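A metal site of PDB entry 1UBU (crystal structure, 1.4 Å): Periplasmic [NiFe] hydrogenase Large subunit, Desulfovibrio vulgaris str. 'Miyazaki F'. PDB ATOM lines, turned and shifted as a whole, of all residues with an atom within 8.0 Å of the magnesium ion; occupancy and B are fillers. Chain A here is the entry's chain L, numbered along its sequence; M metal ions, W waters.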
ATOM      1  N   PHE A  40     -26.559  -6.976  -0.573  1.00  0.00           N
ATOM      2  CA  PHE A  40     -25.337  -7.642  -0.970  1.00  0.00           C
ATOM      3  C   PHE A  40     -24.954  -7.184  -2.401  1.00  0.00           C
ATOM      4  O   PHE A  40     -25.844  -7.044  -3.280  1.00  0.00           O
ATOM      5  CB  PHE A  40     -25.557  -9.161  -0.994  1.00  0.00           C
ATOM      6  CG  PHE A  40     -24.390  -9.961  -1.517  1.00  0.00           C
ATOM      7  CD1 PHE A  40     -23.300 -10.226  -0.697  1.00  0.00           C
ATOM      8  CD2 PHE A  40     -24.372 -10.488  -2.825  1.00  0.00           C
ATOM      9  CE1 PHE A  40     -22.215 -10.965  -1.142  1.00  0.00           C
ATOM     10  CE2 PHE A  40     -23.292 -11.246  -3.258  1.00  0.00           C
ATOM     11  CZ  PHE A  40     -22.228 -11.537  -2.423  1.00  0.00           C
ATOM     12  N   GLU A  44     -16.208  -9.244  -3.851  1.00  0.00           N
ATOM     13  CA  GLU A  44     -15.183 -10.293  -3.820  1.00  0.00           C
ATOM     14  C   GLU A  44     -15.356 -11.299  -4.953  1.00  0.00           C
ATOM     15  O   GLU A  44     -14.360 -11.808  -5.474  1.00  0.00           O
ATOM     16  CB  GLU A  44     -15.251 -11.022  -2.471  1.00  0.00           C
ATOM     17  CG  GLU A  44     -14.766 -10.135  -1.313  1.00  0.00           C
ATOM     18  CD  GLU A  44     -15.410 -10.532   0.024  1.00  0.00           C
ATOM     19  OE1 GLU A  44     -16.442 -11.234   0.046  1.00  0.00           O
ATOM     20  OE2 GLU A  44     -14.891 -10.019   1.055  1.00  0.00           O
ATOM     21  N   GLU A 319     -14.036 -15.580   9.663  1.00  0.00           N
ATOM     22  CA  GLU A 319     -15.371 -15.059   9.361  1.00  0.00           C
ATOM     23  C   GLU A 319     -16.429 -16.167   9.277  1.00  0.00           C
ATOM     24  O   GLU A 319     -16.300 -17.063   8.448  1.00  0.00           O
ATOM     25  CB  GLU A 319     -15.346 -14.271   8.057  1.00  0.00           C
ATOM     26  CG  GLU A 319     -14.444 -13.022   8.192  1.00  0.00           C
ATOM     27  CD  GLU A 319     -14.577 -12.211   6.910  1.00  0.00           C
ATOM     28  OE1 GLU A 319     -15.254 -11.129   6.960  1.00  0.00           O
ATOM     29  OE2 GLU A 319     -14.085 -12.632   5.848  1.00  0.00           O
ATOM     30  N   TYR A 326     -25.043 -17.153   3.455  1.00  0.00           N
ATOM     31  CA  TYR A 326     -24.008 -17.788   2.655  1.00  0.00           C
ATOM     32  C   TYR A 326     -24.117 -19.306   2.857  1.00  0.00           C
ATOM     33  O   TYR A 326     -24.773 -19.757   3.813  1.00  0.00           O
ATOM     34  CB  TYR A 326     -22.559 -17.330   2.983  1.00  0.00           C
ATOM     35  CG  TYR A 326     -22.447 -15.846   2.796  1.00  0.00           C
ATOM     36  CD1 TYR A 326     -22.571 -14.961   3.881  1.00  0.00           C
ATOM     37  CD2 TYR A 326     -22.240 -15.309   1.517  1.00  0.00           C
ATOM     38  CE1 TYR A 326     -22.474 -13.598   3.675  1.00  0.00           C
ATOM     39  CE2 TYR A 326     -22.150 -13.932   1.295  1.00  0.00           C
ATOM     40  CZ  TYR A 326     -22.267 -13.096   2.374  1.00  0.00           C
ATOM     41  OH  TYR A 326     -22.188 -11.727   2.169  1.00  0.00           O
ATOM     42  N   PRO A 334      -9.527 -15.253   6.205  1.00  0.00           N
ATOM     43  CA  PRO A 334      -9.733 -14.624   4.896  1.00  0.00           C
ATOM     44  C   PRO A 334      -8.748 -15.067   3.833  1.00  0.00           C
ATOM     45  O   PRO A 334      -9.106 -14.914   2.658  1.00  0.00           O
ATOM     46  CB  PRO A 334      -9.564 -13.132   5.171  1.00  0.00           C
ATOM     47  CG  PRO A 334      -9.442 -12.968   6.619  1.00  0.00           C
ATOM     48  CD  PRO A 334      -9.369 -14.290   7.296  1.00  0.00           C
ATOM     49  N   GLY A 337     -10.858 -17.514   2.365  1.00  0.00           N
ATOM     50  CA  GLY A 337     -12.248 -17.076   2.458  1.00  0.00           C
ATOM     51  C   GLY A 337     -13.092 -17.607   1.311  1.00  0.00           C
ATOM     52  O   GLY A 337     -12.613 -18.033   0.244  1.00  0.00           O
ATOM     53  N   GLN A 338     -14.407 -17.516   1.607  1.00  0.00           N
ATOM     54  CA  GLN A 338     -15.431 -17.970   0.694  1.00  0.00           C
ATOM     55  C   GLN A 338     -16.598 -16.991   0.688  1.00  0.00           C
ATOM     56  O   GLN A 338     -16.995 -16.578   1.791  1.00  0.00           O
ATOM     57  CB  GLN A 338     -16.037 -19.340   1.082  1.00  0.00           C
ATOM     58  CG  GLN A 338     -14.947 -20.421   0.980  1.00  0.00           C
ATOM     59  CD  GLN A 338     -15.555 -21.781   1.315  1.00  0.00           C
ATOM     60  OE1 GLN A 338     -15.435 -22.724   0.526  1.00  0.00           O
ATOM     61  NE2 GLN A 338     -16.167 -21.834   2.493  1.00  0.00           N
ATOM     62  N   THR A 339     -17.050 -16.646  -0.505  1.00  0.00           N
ATOM     63  CA  THR A 339     -18.236 -15.758  -0.570  1.00  0.00           C
ATOM     64  C   THR A 339     -19.239 -16.391  -1.524  1.00  0.00           C
ATOM     65  O   THR A 339     -19.197 -16.210  -2.748  1.00  0.00           O
ATOM     66  CB  THR A 339     -17.790 -14.380  -1.041  1.00  0.00           C
ATOM     67  OG1 THR A 339     -16.753 -13.953  -0.132  1.00  0.00           O
ATOM     68  CG2 THR A 339     -18.934 -13.380  -0.959  1.00  0.00           C
ATOM     69  N   TRP A 354     -26.578 -10.228   5.408  1.00  0.00           N
ATOM     70  CA  TRP A 354     -25.586 -10.422   4.360  1.00  0.00           C
ATOM     71  C   TRP A 354     -24.171 -10.175   4.872  1.00  0.00           C
ATOM     72  O   TRP A 354     -23.222 -10.412   4.114  1.00  0.00           O
ATOM     73  CB  TRP A 354     -25.833  -9.513   3.154  1.00  0.00           C
ATOM     74  CG  TRP A 354     -27.039  -9.903   2.346  1.00  0.00           C
ATOM     75  CD1 TRP A 354     -28.262  -9.288   2.223  1.00  0.00           C
ATOM     76  CD2 TRP A 354     -27.141 -11.066   1.490  1.00  0.00           C
ATOM     77  NE1 TRP A 354     -29.097  -9.979   1.368  1.00  0.00           N
ATOM     78  CE2 TRP A 354     -28.422 -11.072   0.907  1.00  0.00           C
ATOM     79  CE3 TRP A 354     -26.228 -12.094   1.189  1.00  0.00           C
ATOM     80  CZ2 TRP A 354     -28.804 -12.111   0.019  1.00  0.00           C
ATOM     81  CZ3 TRP A 354     -26.592 -13.112   0.316  1.00  0.00           C
ATOM     82  CH2 TRP A 354     -27.887 -13.094  -0.241  1.00  0.00           C
ATOM     83  N   MET A 355     -24.009  -9.698   6.130  1.00  0.00           N
ATOM     84  CA  MET A 355     -22.644  -9.634   6.640  1.00  0.00           C
ATOM     85  C   MET A 355     -22.190 -10.976   7.200  1.00  0.00           C
ATOM     86  O   MET A 355     -22.968 -11.711   7.821  1.00  0.00           O
ATOM     87  CB  MET A 355     -22.558  -8.654   7.818  1.00  0.00           C
ATOM     88  CG  MET A 355     -22.649  -7.193   7.370  1.00  0.00           C
ATOM     89  SD  MET A 355     -22.044  -6.153   8.745  1.00  0.00           S
ATOM     90  CE  MET A 355     -22.738  -4.539   8.286  1.00  0.00           C
ATOM     91  N   LYS A 356     -20.910 -11.289   6.974  1.00  0.00           N
ATOM     92  CA  LYS A 356     -20.277 -12.405   7.706  1.00  0.00           C
ATOM     93  C   LYS A 356     -20.052 -11.930   9.124  1.00  0.00           C
ATOM     94  O   LYS A 356     -20.237 -10.747   9.418  1.00  0.00           O
ATOM     95  CB  LYS A 356     -18.953 -12.745   7.051  1.00  0.00           C
ATOM     96  CG  LYS A 356     -19.099 -13.225   5.603  1.00  0.00           C
ATOM     97  CD  LYS A 356     -17.731 -13.479   4.947  1.00  0.00           C
ATOM     98  CE  LYS A 356     -17.887 -13.999   3.508  1.00  0.00           C
ATOM     99  NZ  LYS A 356     -16.520 -13.991   2.852  1.00  0.00           N
ATOM    100  N   PRO A 358     -17.160 -11.786  11.703  1.00  0.00           N
ATOM    101  CA  PRO A 358     -15.747 -11.996  12.043  1.00  0.00           C
ATOM    102  C   PRO A 358     -15.600 -12.209  13.539  1.00  0.00           C
ATOM    103  O   PRO A 358     -16.256 -11.562  14.361  1.00  0.00           O
ATOM    104  CB  PRO A 358     -15.097 -10.687  11.631  1.00  0.00           C
ATOM    105  CG  PRO A 358     -16.053 -10.042  10.662  1.00  0.00           C
ATOM    106  CD  PRO A 358     -17.427 -10.408  11.280  1.00  0.00           C
ATOM    107  N   SER A 465      -9.128  -4.823   6.725  1.00  0.00           N
ATOM    108  CA  SER A 465      -8.042  -5.594   6.141  1.00  0.00           C
ATOM    109  C   SER A 465      -8.526  -6.168   4.812  1.00  0.00           C
ATOM    110  O   SER A 465      -9.664  -6.603   4.672  1.00  0.00           O
ATOM    111  CB  SER A 465      -7.567  -6.697   7.080  1.00  0.00           C
ATOM    112  OG  SER A 465      -8.648  -7.509   7.551  1.00  0.00           O
ATOM    113  N   TRP A 467      -7.233  -8.947   1.820  1.00  0.00           N
ATOM    114  CA  TRP A 467      -6.413 -10.146   1.746  1.00  0.00           C
ATOM    115  C   TRP A 467      -6.393 -10.708   0.321  1.00  0.00           C
ATOM    116  O   TRP A 467      -7.486 -10.943  -0.234  1.00  0.00           O
ATOM    117  CB  TRP A 467      -7.000 -11.182   2.706  1.00  0.00           C
ATOM    118  CG  TRP A 467      -7.212 -10.709   4.114  1.00  0.00           C
ATOM    119  CD1 TRP A 467      -8.164  -9.879   4.619  1.00  0.00           C
ATOM    120  CD2 TRP A 467      -6.365 -11.103   5.209  1.00  0.00           C
ATOM    121  NE1 TRP A 467      -7.960  -9.733   5.980  1.00  0.00           N
ATOM    122  CE2 TRP A 467      -6.860 -10.485   6.349  1.00  0.00           C
ATOM    123  CE3 TRP A 467      -5.233 -11.935   5.328  1.00  0.00           C
ATOM    124  CZ2 TRP A 467      -6.264 -10.661   7.592  1.00  0.00           C
ATOM    125  CZ3 TRP A 467      -4.623 -12.127   6.551  1.00  0.00           C
ATOM    126  CH2 TRP A 467      -5.151 -11.479   7.682  1.00  0.00           C
ATOM    127  N   PHE A 478      -9.766 -12.766  -3.224  1.00  0.00           N
ATOM    128  CA  PHE A 478      -9.612 -11.402  -2.675  1.00  0.00           C
ATOM    129  C   PHE A 478     -10.722 -11.302  -1.616  1.00  0.00           C
ATOM    130  O   PHE A 478     -11.888 -11.483  -1.955  1.00  0.00           O
ATOM    131  CB  PHE A 478      -9.727 -10.323  -3.714  1.00  0.00           C
ATOM    132  CG  PHE A 478      -9.058  -9.022  -3.284  1.00  0.00           C
ATOM    133  CD1 PHE A 478      -9.696  -8.243  -2.294  1.00  0.00           C
ATOM    134  CD2 PHE A 478      -7.866  -8.592  -3.796  1.00  0.00           C
ATOM    135  CE1 PHE A 478      -9.106  -7.078  -1.863  1.00  0.00           C
ATOM    136  CE2 PHE A 478      -7.269  -7.400  -3.371  1.00  0.00           C
ATOM    137  CZ  PHE A 478      -7.888  -6.627  -2.383  1.00  0.00           C
ATOM    138  N   GLN A 479     -10.326 -11.067  -0.370  1.00  0.00           N
ATOM    139  CA  GLN A 479     -11.310 -11.009   0.711  1.00  0.00           C
ATOM    140  C   GLN A 479     -11.152  -9.680   1.440  1.00  0.00           C
ATOM    141  O   GLN A 479     -10.044  -9.303   1.813  1.00  0.00           O
ATOM    142  CB  GLN A 479     -11.106 -12.192   1.656  1.00  0.00           C
ATOM    143  CG  GLN A 479     -11.473 -13.562   1.070  1.00  0.00           C
ATOM    144  CD  GLN A 479     -12.944 -13.688   0.760  1.00  0.00           C
ATOM    145  OE1 GLN A 479     -13.826 -13.243   1.526  1.00  0.00           O
ATOM    146  NE2 GLN A 479     -13.229 -14.348  -0.353  1.00  0.00           N
ATOM    147  N   LEU A 480     -12.286  -9.019   1.652  1.00  0.00           N
ATOM    148  CA  LEU A 480     -12.364  -7.821   2.489  1.00  0.00           C
ATOM    149  C   LEU A 480     -12.952  -8.176   3.846  1.00  0.00           C
ATOM    150  O   LEU A 480     -13.968  -8.816   3.861  1.00  0.00           O
ATOM    151  CB  LEU A 480     -13.238  -6.711   1.883  1.00  0.00           C
ATOM    152  CG  LEU A 480     -12.941  -6.224   0.450  1.00  0.00           C
ATOM    153  CD1 LEU A 480     -13.540  -4.810   0.338  1.00  0.00           C
ATOM    154  CD2 LEU A 480     -11.528  -6.183   0.152  1.00  0.00           C
ATOM    155  N   VAL A 481     -12.330  -7.761   4.956  1.00  0.00           N
ATOM    156  CA  VAL A 481     -12.889  -7.925   6.294  1.00  0.00           C
ATOM    157  C   VAL A 481     -12.905  -6.498   6.830  1.00  0.00           C
ATOM    158  O   VAL A 481     -11.865  -5.900   7.016  1.00  0.00           O
ATOM    159  CB  VAL A 481     -12.036  -8.814   7.193  1.00  0.00           C
ATOM    160  CG1 VAL A 481     -12.761  -9.051   8.516  1.00  0.00           C
ATOM    161  CG2 VAL A 481     -11.715 -10.101   6.467  1.00  0.00           C
ATOM    162  N   VAL A 482     -14.117  -5.960   7.004  1.00  0.00           N
ATOM    163  CA  VAL A 482     -14.210  -4.507   7.110  1.00  0.00           C
ATOM    164  C   VAL A 482     -14.675  -4.115   8.501  1.00  0.00           C
ATOM    165  O   VAL A 482     -15.336  -4.962   9.158  1.00  0.00           O
ATOM    166  CB  VAL A 482     -15.183  -4.038   6.003  1.00  0.00           C
ATOM    167  CG1 VAL A 482     -15.282  -2.545   5.884  1.00  0.00           C
ATOM    168  CG2 VAL A 482     -14.721  -4.526   4.645  1.00  0.00           C
ATOM    169  N   THR A 485     -18.131  -4.928   9.472  1.00  0.00           N
ATOM    170  CA  THR A 485     -18.373  -6.361   9.536  1.00  0.00           C
ATOM    171  C   THR A 485     -18.138  -6.881  10.965  1.00  0.00           C
ATOM    172  O   THR A 485     -18.961  -7.635  11.486  1.00  0.00           O
ATOM    173  CB  THR A 485     -17.455  -7.107   8.548  1.00  0.00           C
ATOM    174  OG1 THR A 485     -17.264  -6.414   7.306  1.00  0.00           O
ATOM    175  CG2 THR A 485     -18.055  -8.491   8.227  1.00  0.00           C
ATOM    176  N   CYS A 531     -19.855  -1.095   3.354  1.00  0.00           N
ATOM    177  CA  CYS A 531     -18.585  -1.576   3.888  1.00  0.00           C
ATOM    178  C   CYS A 531     -18.728  -2.977   4.470  1.00  0.00           C
ATOM    179  O   CYS A 531     -17.959  -3.885   4.171  1.00  0.00           O
ATOM    180  CB  CYS A 531     -18.057  -0.667   4.993  1.00  0.00           C
ATOM    181  SG  CYS A 531     -16.933   0.606   4.369  1.00  0.00           S
ATOM    182  N   GLY A 532     -19.721  -3.162   5.359  1.00  0.00           N
ATOM    183  CA  GLY A 532     -19.745  -4.434   6.082  1.00  0.00           C
ATOM    184  C   GLY A 532     -19.974  -5.644   5.208  1.00  0.00           C
ATOM    185  O   GLY A 532     -19.429  -6.729   5.488  1.00  0.00           O
ATOM    186  N   VAL A 533     -20.811  -5.455   4.174  1.00  0.00           N
ATOM    187  CA  VAL A 533     -21.180  -6.564   3.291  1.00  0.00           C
ATOM    188  C   VAL A 533     -20.391  -6.676   2.014  1.00  0.00           C
ATOM    189  O   VAL A 533     -19.982  -7.765   1.600  1.00  0.00           O
ATOM    190  CB  VAL A 533     -22.639  -6.453   2.824  1.00  0.00           C
ATOM    191  CG1 VAL A 533     -23.029  -7.583   1.889  1.00  0.00           C
ATOM    192  CG2 VAL A 533     -23.554  -6.480   4.035  1.00  0.00           C
ATOM    193  N   HIS A 534     -20.087  -5.537   1.353  1.00  0.00           N
ATOM    194  CA  HIS A 534     -19.375  -5.479   0.082  1.00  0.00           C
ATOM    195  C   HIS A 534     -19.887  -6.545  -0.908  1.00  0.00           C
ATOM    196  O   HIS A 534     -21.195  -6.599  -0.977  1.00  0.00           O
ATOM    197  CB  HIS A 534     -17.850  -5.526   0.215  1.00  0.00           C
ATOM    198  CG  HIS A 534     -17.279  -6.450   1.230  1.00  0.00           C
ATOM    199  ND1 HIS A 534     -17.304  -6.115   2.606  1.00  0.00           N
ATOM    200  CD2 HIS A 534     -16.808  -7.704   1.146  1.00  0.00           C
ATOM    201  CE1 HIS A 534     -16.806  -7.134   3.257  1.00  0.00           C
ATOM    202  NE2 HIS A 534     -16.489  -8.098   2.402  1.00  0.00           N
ATOM    203  OXT HIS A 534     -19.161  -7.240  -1.599  1.00  0.00           O
HETATM  204 MG    MG M   1     -15.618  -9.957   3.067  1.00  0.00          MG
HETATM  205  O   HOH W   1     -16.501  -9.964   4.924  1.00  0.00           O
HETATM  206  O   HOH W   2     -17.317 -11.062   2.600  1.00  0.00           O
HETATM  207  O   HOH W   3     -14.652 -11.681   3.673  1.00  0.00           O
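Water W2 lies within hydrogen-bond range of OE1 of Glu 44 (2.7 Å) and NZ of Lys 356 (3.0 Å). Water W3 lies within hydrogen-bond range of the side-chain carboxylate (OE2) of Glu 319 (2.4 Å), the side-chain amide oxygen (OE1) of Gln 479 (2.8 Å) and the side-chain amino group (NZ) of Lys 356 (3.1 Å).
OG1 of Thr 339 lies within hydrogen-bond range of OE1 of Glu 44 (2.7 Å). OE1 of Glu 44 is in salt-bridge range of NZ of Lys 356. OE1 of Gln 479 sits close to OE2 of Glu 44 (3.4 Å). ND1 of His 534 is in hydrogen-bond range of O of Cys 531 (2.8 Å).
The magnesium ion is bound by water W1, at 2.1 Å. The magnesium ion is bound by water W3 (2.1 Å). Water W2 is bound to the magnesium ion. The magnesium ion is bound by the side-chain carboxylate (OE2) of Glu 44 (2.1 Å). O of Leu 480 binds the magnesium ion (2.2 Å). NE2 of His 534 binds the magnesium ion (2.2 Å). The magnesium ion has six donor atoms within binding distance.
Three residues have an atom within 4 Å of the magnesium ion: Glu 44, Leu 480 and His 534.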
